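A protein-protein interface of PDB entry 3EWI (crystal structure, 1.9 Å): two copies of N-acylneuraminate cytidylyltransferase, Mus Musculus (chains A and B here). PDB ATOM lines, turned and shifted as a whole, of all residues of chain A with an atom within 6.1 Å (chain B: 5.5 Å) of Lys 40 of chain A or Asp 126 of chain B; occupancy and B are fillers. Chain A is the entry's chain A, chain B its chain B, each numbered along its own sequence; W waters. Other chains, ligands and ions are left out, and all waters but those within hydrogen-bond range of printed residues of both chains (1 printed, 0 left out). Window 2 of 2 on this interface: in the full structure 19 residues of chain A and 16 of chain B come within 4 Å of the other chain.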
ATOM      1  N   ASP A  38       6.331 -10.676 -23.462  1.00  0.00           N
ATOM      2  CA  ASP A  38       5.500 -10.304 -22.306  1.00  0.00           C
ATOM      3  C   ASP A  38       4.749 -11.540 -21.835  1.00  0.00           C
ATOM      4  O   ASP A  38       4.121 -12.245 -22.635  1.00  0.00           O
ATOM      5  CB  ASP A  38       4.495  -9.216 -22.720  1.00  0.00           C
ATOM      6  CG  ASP A  38       3.900  -8.464 -21.544  1.00  0.00           C
ATOM      7  OD1 ASP A  38       3.555  -9.086 -20.510  1.00  0.00           O
ATOM      8  OD2 ASP A  38       3.734  -7.239 -21.692  1.00  0.00           O
ATOM      9  N   VAL A  39       4.845 -11.810 -20.540  1.00  0.00           N
ATOM     10  CA  VAL A  39       4.118 -12.896 -19.872  1.00  0.00           C
ATOM     11  C   VAL A  39       2.597 -12.846 -20.141  1.00  0.00           C
ATOM     12  O   VAL A  39       1.966 -13.886 -20.341  1.00  0.00           O
ATOM     13  CB  VAL A  39       4.460 -12.910 -18.360  1.00  0.00           C
ATOM     14  CG1 VAL A  39       3.566 -13.839 -17.604  1.00  0.00           C
ATOM     15  CG2 VAL A  39       5.879 -13.361 -18.176  1.00  0.00           C
ATOM     16  N   LYS A  40       2.036 -11.634 -20.157  1.00  0.00           N
ATOM     17  CA  LYS A  40       0.639 -11.400 -20.546  1.00  0.00           C
ATOM     18  C   LYS A  40       0.297 -12.153 -21.842  1.00  0.00           C
ATOM     19  O   LYS A  40      -0.772 -12.727 -21.956  1.00  0.00           O
ATOM     20  CB  LYS A  40       0.411  -9.909 -20.821  1.00  0.00           C
ATOM     21  CG  LYS A  40      -0.191  -9.165 -19.681  1.00  0.00           C
ATOM     22  CD  LYS A  40      -0.363  -7.675 -20.020  1.00  0.00           C
ATOM     23  CE  LYS A  40      -1.147  -7.010 -18.897  1.00  0.00           C
ATOM     24  NZ  LYS A  40      -1.131  -5.516 -18.901  1.00  0.00           N
ATOM     25  N   ASP A  41       1.225 -12.118 -22.797  1.00  0.00           N
ATOM     26  CA  ASP A  41       1.000 -12.689 -24.146  1.00  0.00           C
ATOM     27  C   ASP A  41       1.125 -14.197 -24.159  1.00  0.00           C
ATOM     28  O   ASP A  41       0.335 -14.889 -24.815  1.00  0.00           O
ATOM     29  CB  ASP A  41       1.989 -12.067 -25.133  1.00  0.00           C
ATOM     30  CG  ASP A  41       1.733 -10.608 -25.352  1.00  0.00           C
ATOM     31  OD1 ASP A  41       0.569 -10.218 -25.232  1.00  0.00           O
ATOM     32  OD2 ASP A  41       2.675  -9.848 -25.661  1.00  0.00           O
ATOM     33  N   ALA A  42       2.124 -14.713 -23.442  1.00  0.00           N
ATOM     34  CA  ALA A  42       2.258 -16.156 -23.217  1.00  0.00           C
ATOM     35  C   ALA A  42       1.015 -16.748 -22.548  1.00  0.00           C
ATOM     36  O   ALA A  42       0.531 -17.815 -22.933  1.00  0.00           O
ATOM     37  CB  ALA A  42       3.530 -16.463 -22.399  1.00  0.00           C
ATOM     38  N   ILE A  43       0.478 -16.051 -21.555  1.00  0.00           N
ATOM     39  CA  ILE A  43      -0.733 -16.514 -20.886  1.00  0.00           C
ATOM     40  C   ILE A  43      -1.948 -16.370 -21.820  1.00  0.00           C
ATOM     41  O   ILE A  43      -2.877 -17.161 -21.751  1.00  0.00           O
ATOM     42  CB  ILE A  43      -0.959 -15.764 -19.544  1.00  0.00           C
ATOM     43  CG1 ILE A  43       0.101 -16.200 -18.518  1.00  0.00           C
ATOM     44  CG2 ILE A  43      -2.376 -16.010 -19.010  1.00  0.00           C
ATOM     45  CD1 ILE A  43       0.337 -15.188 -17.366  1.00  0.00           C
ATOM     46  N   GLY A  44      -1.920 -15.354 -22.687  1.00  0.00           N
ATOM     47  CA  GLY A  44      -2.993 -15.145 -23.648  1.00  0.00           C
ATOM     48  C   GLY A  44      -3.034 -16.372 -24.548  1.00  0.00           C
ATOM     49  O   GLY A  44      -4.107 -16.913 -24.830  1.00  0.00           O
ATOM     50  N   ILE A  45      -1.850 -16.846 -24.927  1.00  0.00           N
ATOM     51  CA  ILE A  45      -1.742 -18.043 -25.773  1.00  0.00           C
ATOM     52  C   ILE A  45      -2.254 -19.262 -24.993  1.00  0.00           C
ATOM     53  O   ILE A  45      -3.052 -20.046 -25.514  1.00  0.00           O
ATOM     54  CB  ILE A  45      -0.294 -18.195 -26.332  1.00  0.00           C
ATOM     55  CG1 ILE A  45      -0.016 -17.030 -27.292  1.00  0.00           C
ATOM     56  CG2 ILE A  45      -0.073 -19.586 -26.942  1.00  0.00           C
ATOM     57  CD1 ILE A  45       1.437 -16.869 -27.789  1.00  0.00           C
ATOM     58  N   ARG A 145       4.501  -6.800 -26.197  1.00  0.00           N
ATOM     59  CA  ARG A 145       4.128  -6.051 -24.986  1.00  0.00           C
ATOM     60  C   ARG A 145       2.606  -5.993 -24.798  1.00  0.00           C
ATOM     61  O   ARG A 145       2.035  -4.962 -24.409  1.00  0.00           O
ATOM     62  CB  ARG A 145       4.728  -4.644 -25.041  1.00  0.00           C
ATOM     63  CG  ARG A 145       6.243  -4.615 -24.991  1.00  0.00           C
ATOM     64  CD  ARG A 145       6.759  -5.168 -23.666  1.00  0.00           C
ATOM     65  NE  ARG A 145       8.201  -5.005 -23.442  1.00  0.00           N
ATOM     66  CZ  ARG A 145       9.115  -5.958 -23.582  1.00  0.00           C
ATOM     67  NH1 ARG A 145       8.763  -7.171 -23.971  1.00  0.00           N
ATOM     68  NH2 ARG A 145      10.400  -5.706 -23.307  1.00  0.00           N
ATOM     69  N   GLY A 146       1.942  -7.111 -25.071  1.00  0.00           N
ATOM     70  CA  GLY A 146       0.550  -7.257 -24.675  1.00  0.00           C
ATOM     71  C   GLY A 146      -0.453  -7.360 -25.828  1.00  0.00           C
ATOM     72  O   GLY A 146      -1.636  -7.506 -25.591  1.00  0.00           O
ATOM     73  N   ILE A 148      -0.779  -9.661 -28.272  1.00  0.00           N
ATOM     74  CA  ILE A 148      -1.379 -10.994 -28.373  1.00  0.00           C
ATOM     75  C   ILE A 148      -2.472 -11.172 -27.288  1.00  0.00           C
ATOM     76  O   ILE A 148      -3.529 -11.710 -27.579  1.00  0.00           O
ATOM     77  CB  ILE A 148      -0.336 -12.140 -28.262  1.00  0.00           C
ATOM     78  CG1 ILE A 148       0.583 -12.199 -29.500  1.00  0.00           C
ATOM     79  CG2 ILE A 148      -1.034 -13.473 -28.035  1.00  0.00           C
ATOM     80  CD1 ILE A 148       1.874 -13.026 -29.287  1.00  0.00           C
ATOM     81  N   ARG A 149      -2.225 -10.715 -26.051  1.00  0.00           N
ATOM     82  CA  ARG A 149      -3.228 -10.867 -24.993  1.00  0.00           C
ATOM     83  C   ARG A 149      -4.465 -10.030 -25.311  1.00  0.00           C
ATOM     84  O   ARG A 149      -5.584 -10.439 -25.049  1.00  0.00           O
ATOM     85  CB  ARG A 149      -2.642 -10.473 -23.595  1.00  0.00           C
ATOM     86  CG  ARG A 149      -3.593 -10.649 -22.439  1.00  0.00           C
ATOM     87  CD  ARG A 149      -4.107 -12.070 -22.287  1.00  0.00           C
ATOM     88  NE  ARG A 149      -4.862 -12.230 -21.055  1.00  0.00           N
ATOM     89  CZ  ARG A 149      -4.297 -12.432 -19.862  1.00  0.00           C
ATOM     90  NH1 ARG A 149      -2.977 -12.528 -19.761  1.00  0.00           N
ATOM     91  NH2 ARG A 149      -5.052 -12.558 -18.785  1.00  0.00           N
ATOM     92  N   GLY B  18       4.349  -9.580 -13.412  1.00  0.00           N
ATOM     93  CA  GLY B  18       3.240  -8.646 -13.472  1.00  0.00           C
ATOM     94  C   GLY B  18       2.918  -7.885 -12.197  1.00  0.00           C
ATOM     95  O   GLY B  18       2.132  -6.937 -12.243  1.00  0.00           O
ATOM     96  N   ASN B  22       7.403  -6.054 -14.319  1.00  0.00           N
ATOM     97  CA  ASN B  22       6.478  -5.492 -15.274  1.00  0.00           C
ATOM     98  C   ASN B  22       5.973  -6.575 -16.225  1.00  0.00           C
ATOM     99  O   ASN B  22       5.214  -6.301 -17.151  1.00  0.00           O
ATOM    100  CB  ASN B  22       7.164  -4.350 -16.035  1.00  0.00           C
ATOM    101  CG  ASN B  22       8.498  -4.751 -16.614  1.00  0.00           C
ATOM    102  OD1 ASN B  22       8.793  -5.941 -16.793  1.00  0.00           O
ATOM    103  ND2 ASN B  22       9.326  -3.770 -16.890  1.00  0.00           N
ATOM    104  N   GLY B  23       6.412  -7.809 -16.002  1.00  0.00           N
ATOM    105  CA  GLY B  23       5.958  -8.935 -16.837  1.00  0.00           C
ATOM    106  C   GLY B  23       6.804  -9.154 -18.084  1.00  0.00           C
ATOM    107  O   GLY B  23       6.626 -10.152 -18.768  1.00  0.00           O
ATOM    108  N   GLU B 108      -3.313 -11.633 -12.531  1.00  0.00           N
ATOM    109  CA  GLU B 108      -3.782 -12.598 -13.534  1.00  0.00           C
ATOM    110  C   GLU B 108      -5.010 -13.410 -13.161  1.00  0.00           C
ATOM    111  O   GLU B 108      -5.390 -13.517 -11.990  1.00  0.00           O
ATOM    112  CB  GLU B 108      -2.639 -13.537 -13.930  1.00  0.00           C
ATOM    113  CG  GLU B 108      -1.786 -12.997 -15.073  1.00  0.00           C
ATOM    114  CD  GLU B 108      -2.574 -12.941 -16.379  1.00  0.00           C
ATOM    115  OE1 GLU B 108      -3.675 -13.514 -16.399  1.00  0.00           O
ATOM    116  OE2 GLU B 108      -2.111 -12.287 -17.336  1.00  0.00           O
ATOM    117  N   PRO B 124      -2.154  -4.306  -9.594  1.00  0.00           N
ATOM    118  CA  PRO B 124      -1.564  -3.149 -10.249  1.00  0.00           C
ATOM    119  C   PRO B 124      -2.479  -2.560 -11.319  1.00  0.00           C
ATOM    120  O   PRO B 124      -3.439  -3.213 -11.753  1.00  0.00           O
ATOM    121  CB  PRO B 124      -0.287  -3.692 -10.896  1.00  0.00           C
ATOM    122  CG  PRO B 124      -0.174  -5.115 -10.500  1.00  0.00           C
ATOM    123  CD  PRO B 124      -1.478  -5.565  -9.957  1.00  0.00           C
ATOM    124  N   ALA B 125      -2.162  -1.339 -11.747  1.00  0.00           N
ATOM    125  CA  ALA B 125      -2.981  -0.599 -12.696  1.00  0.00           C
ATOM    126  C   ALA B 125      -3.202  -1.382 -13.996  1.00  0.00           C
ATOM    127  O   ALA B 125      -4.222  -1.223 -14.649  1.00  0.00           O
ATOM    128  CB  ALA B 125      -2.342   0.746 -12.987  1.00  0.00           C
ATOM    129  N   ASP B 126      -2.235  -2.224 -14.354  1.00  0.00           N
ATOM    130  CA  ASP B 126      -2.254  -2.958 -15.630  1.00  0.00           C
ATOM    131  C   ASP B 126      -2.635  -4.437 -15.514  1.00  0.00           C
ATOM    132  O   ASP B 126      -2.311  -5.239 -16.390  1.00  0.00           O
ATOM    133  CB  ASP B 126      -0.894  -2.819 -16.338  1.00  0.00           C
ATOM    134  CG  ASP B 126       0.286  -3.326 -15.493  1.00  0.00           C
ATOM    135  OD1 ASP B 126       0.160  -3.527 -14.258  1.00  0.00           O
ATOM    136  OD2 ASP B 126       1.366  -3.516 -16.087  1.00  0.00           O
ATOM    137  N   ALA B 127      -3.329  -4.797 -14.442  1.00  0.00           N
ATOM    138  CA  ALA B 127      -3.790  -6.164 -14.254  1.00  0.00           C
ATOM    139  C   ALA B 127      -4.915  -6.458 -15.244  1.00  0.00           C
ATOM    140  O   ALA B 127      -5.569  -5.529 -15.756  1.00  0.00           O
ATOM    141  CB  ALA B 127      -4.283  -6.359 -12.843  1.00  0.00           C
ATOM    142  N   CYS B 128      -5.150  -7.743 -15.502  1.00  0.00           N
ATOM    143  CA  CYS B 128      -6.255  -8.130 -16.351  1.00  0.00           C
ATOM    144  C   CYS B 128      -7.591  -7.725 -15.724  1.00  0.00           C
ATOM    145  O   CYS B 128      -7.722  -7.630 -14.491  1.00  0.00           O
ATOM    146  CB  CYS B 128      -6.212  -9.630 -16.687  1.00  0.00           C
ATOM    147  SG  CYS B 128      -6.739 -10.774 -15.389  1.00  0.00           S
ATOM    148  N   GLN B 132      -8.851  -7.386 -11.652  1.00  0.00           N
ATOM    149  CA  GLN B 132      -9.370  -6.078 -11.223  1.00  0.00           C
ATOM    150  C   GLN B 132     -10.755  -6.156 -10.586  1.00  0.00           C
ATOM    151  O   GLN B 132     -11.007  -5.488  -9.586  1.00  0.00           O
ATOM    152  CB  GLN B 132      -9.413  -5.091 -12.387  1.00  0.00           C
ATOM    153  CG  GLN B 132      -8.059  -4.673 -12.894  1.00  0.00           C
ATOM    154  CD  GLN B 132      -8.118  -3.475 -13.817  1.00  0.00           C
ATOM    155  OE1 GLN B 132      -7.265  -3.312 -14.685  1.00  0.00           O
ATOM    156  NE2 GLN B 132      -9.117  -2.626 -13.633  1.00  0.00           N
ATOM    157  N   CYS B 141      -0.251   2.604  -9.515  1.00  0.00           N
ATOM    158  CA  CYS B 141       0.997   2.086 -10.092  1.00  0.00           C
ATOM    159  C   CYS B 141       0.847   0.731 -10.796  1.00  0.00           C
ATOM    160  O   CYS B 141       0.038  -0.100 -10.399  1.00  0.00           O
ATOM    161  CB  CYS B 141       2.082   1.964  -9.020  1.00  0.00           C
ATOM    162  SG  CYS B 141       2.674   3.545  -8.342  1.00  0.00           S
ATOM    163  N   SER B 142       1.674   0.512 -11.810  1.00  0.00           N
ATOM    164  CA  SER B 142       1.652  -0.732 -12.572  1.00  0.00           C
ATOM    165  C   SER B 142       2.681  -1.700 -12.008  1.00  0.00           C
ATOM    166  O   SER B 142       3.499  -1.310 -11.166  1.00  0.00           O
ATOM    167  CB  SER B 142       1.896  -0.460 -14.056  1.00  0.00           C
ATOM    168  OG  SER B 142       0.952   0.466 -14.567  1.00  0.00           O
ATOM    169  N   GLY B 143       2.616  -2.945 -12.485  1.00  0.00           N
ATOM    170  CA  GLY B 143       3.409  -4.057 -12.007  1.00  0.00           C
ATOM    171  C   GLY B 143       4.850  -3.772 -12.288  1.00  0.00           C
ATOM    172  O   GLY B 143       5.176  -3.245 -13.350  1.00  0.00           O
ATOM    173  N   ARG B 145       6.452  -1.422 -11.157  1.00  0.00           N
ATOM    174  CA  ARG B 145       6.661   0.016 -11.244  1.00  0.00           C
ATOM    175  C   ARG B 145       6.058   0.762 -10.039  1.00  0.00           C
ATOM    176  O   ARG B 145       5.597   1.892 -10.168  1.00  0.00           O
ATOM    177  CB  ARG B 145       6.103   0.566 -12.572  1.00  0.00           C
ATOM    178  CG  ARG B 145       6.484  -0.223 -13.851  1.00  0.00           C
ATOM    179  CD  ARG B 145       5.370  -0.062 -14.884  1.00  0.00           C
ATOM    180  NE  ARG B 145       5.465  -0.882 -16.102  1.00  0.00           N
ATOM    181  CZ  ARG B 145       4.729  -1.966 -16.370  1.00  0.00           C
ATOM    182  NH1 ARG B 145       3.850  -2.448 -15.501  1.00  0.00           N
ATOM    183  NH2 ARG B 145       4.889  -2.596 -17.520  1.00  0.00           N
HETATM  184  O   HOH W   1       3.351  -7.691 -18.363  1.00  0.00           O
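The backbone NH (N) of Val 39 of chain A lies within hydrogen-bond range of the backbone carbonyl oxygen (O) of Gly 23 of chain B, 3.0 Å away. NZ of Lys 40 of chain A is in hydrogen-bond range of O of Asp 126 of chain B, 2.8 Å away. The guanidinium group (NH1) of Arg 149 of chain A lies within salt-bridge range of the side-chain carboxylate (OE2) of Glu 108 of chain B (2.6 Å).
N of Gly 143 of chain B is in hydrogen-bond range of OD1 of Asp 126 of chain B (3.1 Å). O of Lys 40 of chain A is in hydrogen-bond range of NH1 of Arg 149 of chain A, 3.1 Å away. The side-chain carboxylate (OD2) of Asp 126 of chain B is in salt-bridge range of the guanidinium group (NH1) of Arg 145 of chain B (2.8 Å). The side-chain carboxylate of Asp 38 of chain A is in hydrogen-bond range of the backbone NH of Lys 40 of chain A (3.0 Å). The side-chain carboxylate (OD1) of Asp 41 of chain A is in hydrogen-bond range of the backbone NH (N) of Arg 149 of chain A, at 3.0 Å.
Asp 38 of chain A touches Gly 23 of chain B (OD1 to O, 3.7 Å). OE2 of Glu 108 of chain B touches CD1 of Ile 43 of chain A, 3.8 Å away. Arg 149 of chain A touches Cys 128 of chain B (NH2 to CB, 3.8 Å).
Printed residues of chain B within 4 Å of Asp 38 of chain A: Gly 23. Of chain B, only Asp 126 comes within 4 Å of Lys 40 of chain A. Of the printed residues of chain B, Ile 43 of chain A touches Glu 108 (3.8 Å). Printed residues of chain B within 4 Å of Arg 149 of chain A: Glu 108 (2.6 Å) and Cys 128 (3.8 Å). Of chain A, only Lys 40 comes within 4 Å of Asp 126 of chain B. Printed residues of chain A within 4 Å of Cys 128 of chain B: Arg 149. Arg 145 of chain B touches none of the printed residues of chain A. The nearest printed residue of chain A that does not touch Gly 23 of chain B is Lys 40 of chain A (5.0 Å).
Of the 12 printed residues of chain A, 5 touch a printed residue of chain B. Hydrophobic or aromatic side chains of chain A that line the printed part of chain B: Val 39 and Ile 43. Along chain B the printed residues that touch a printed residue of chain A span positions 23 to 128.
Position printed for both chains: 145.
Water W1 lies within hydrogen-bond range of OD1 of Asp 38 of chain A and O of Asn 22 of chain B.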
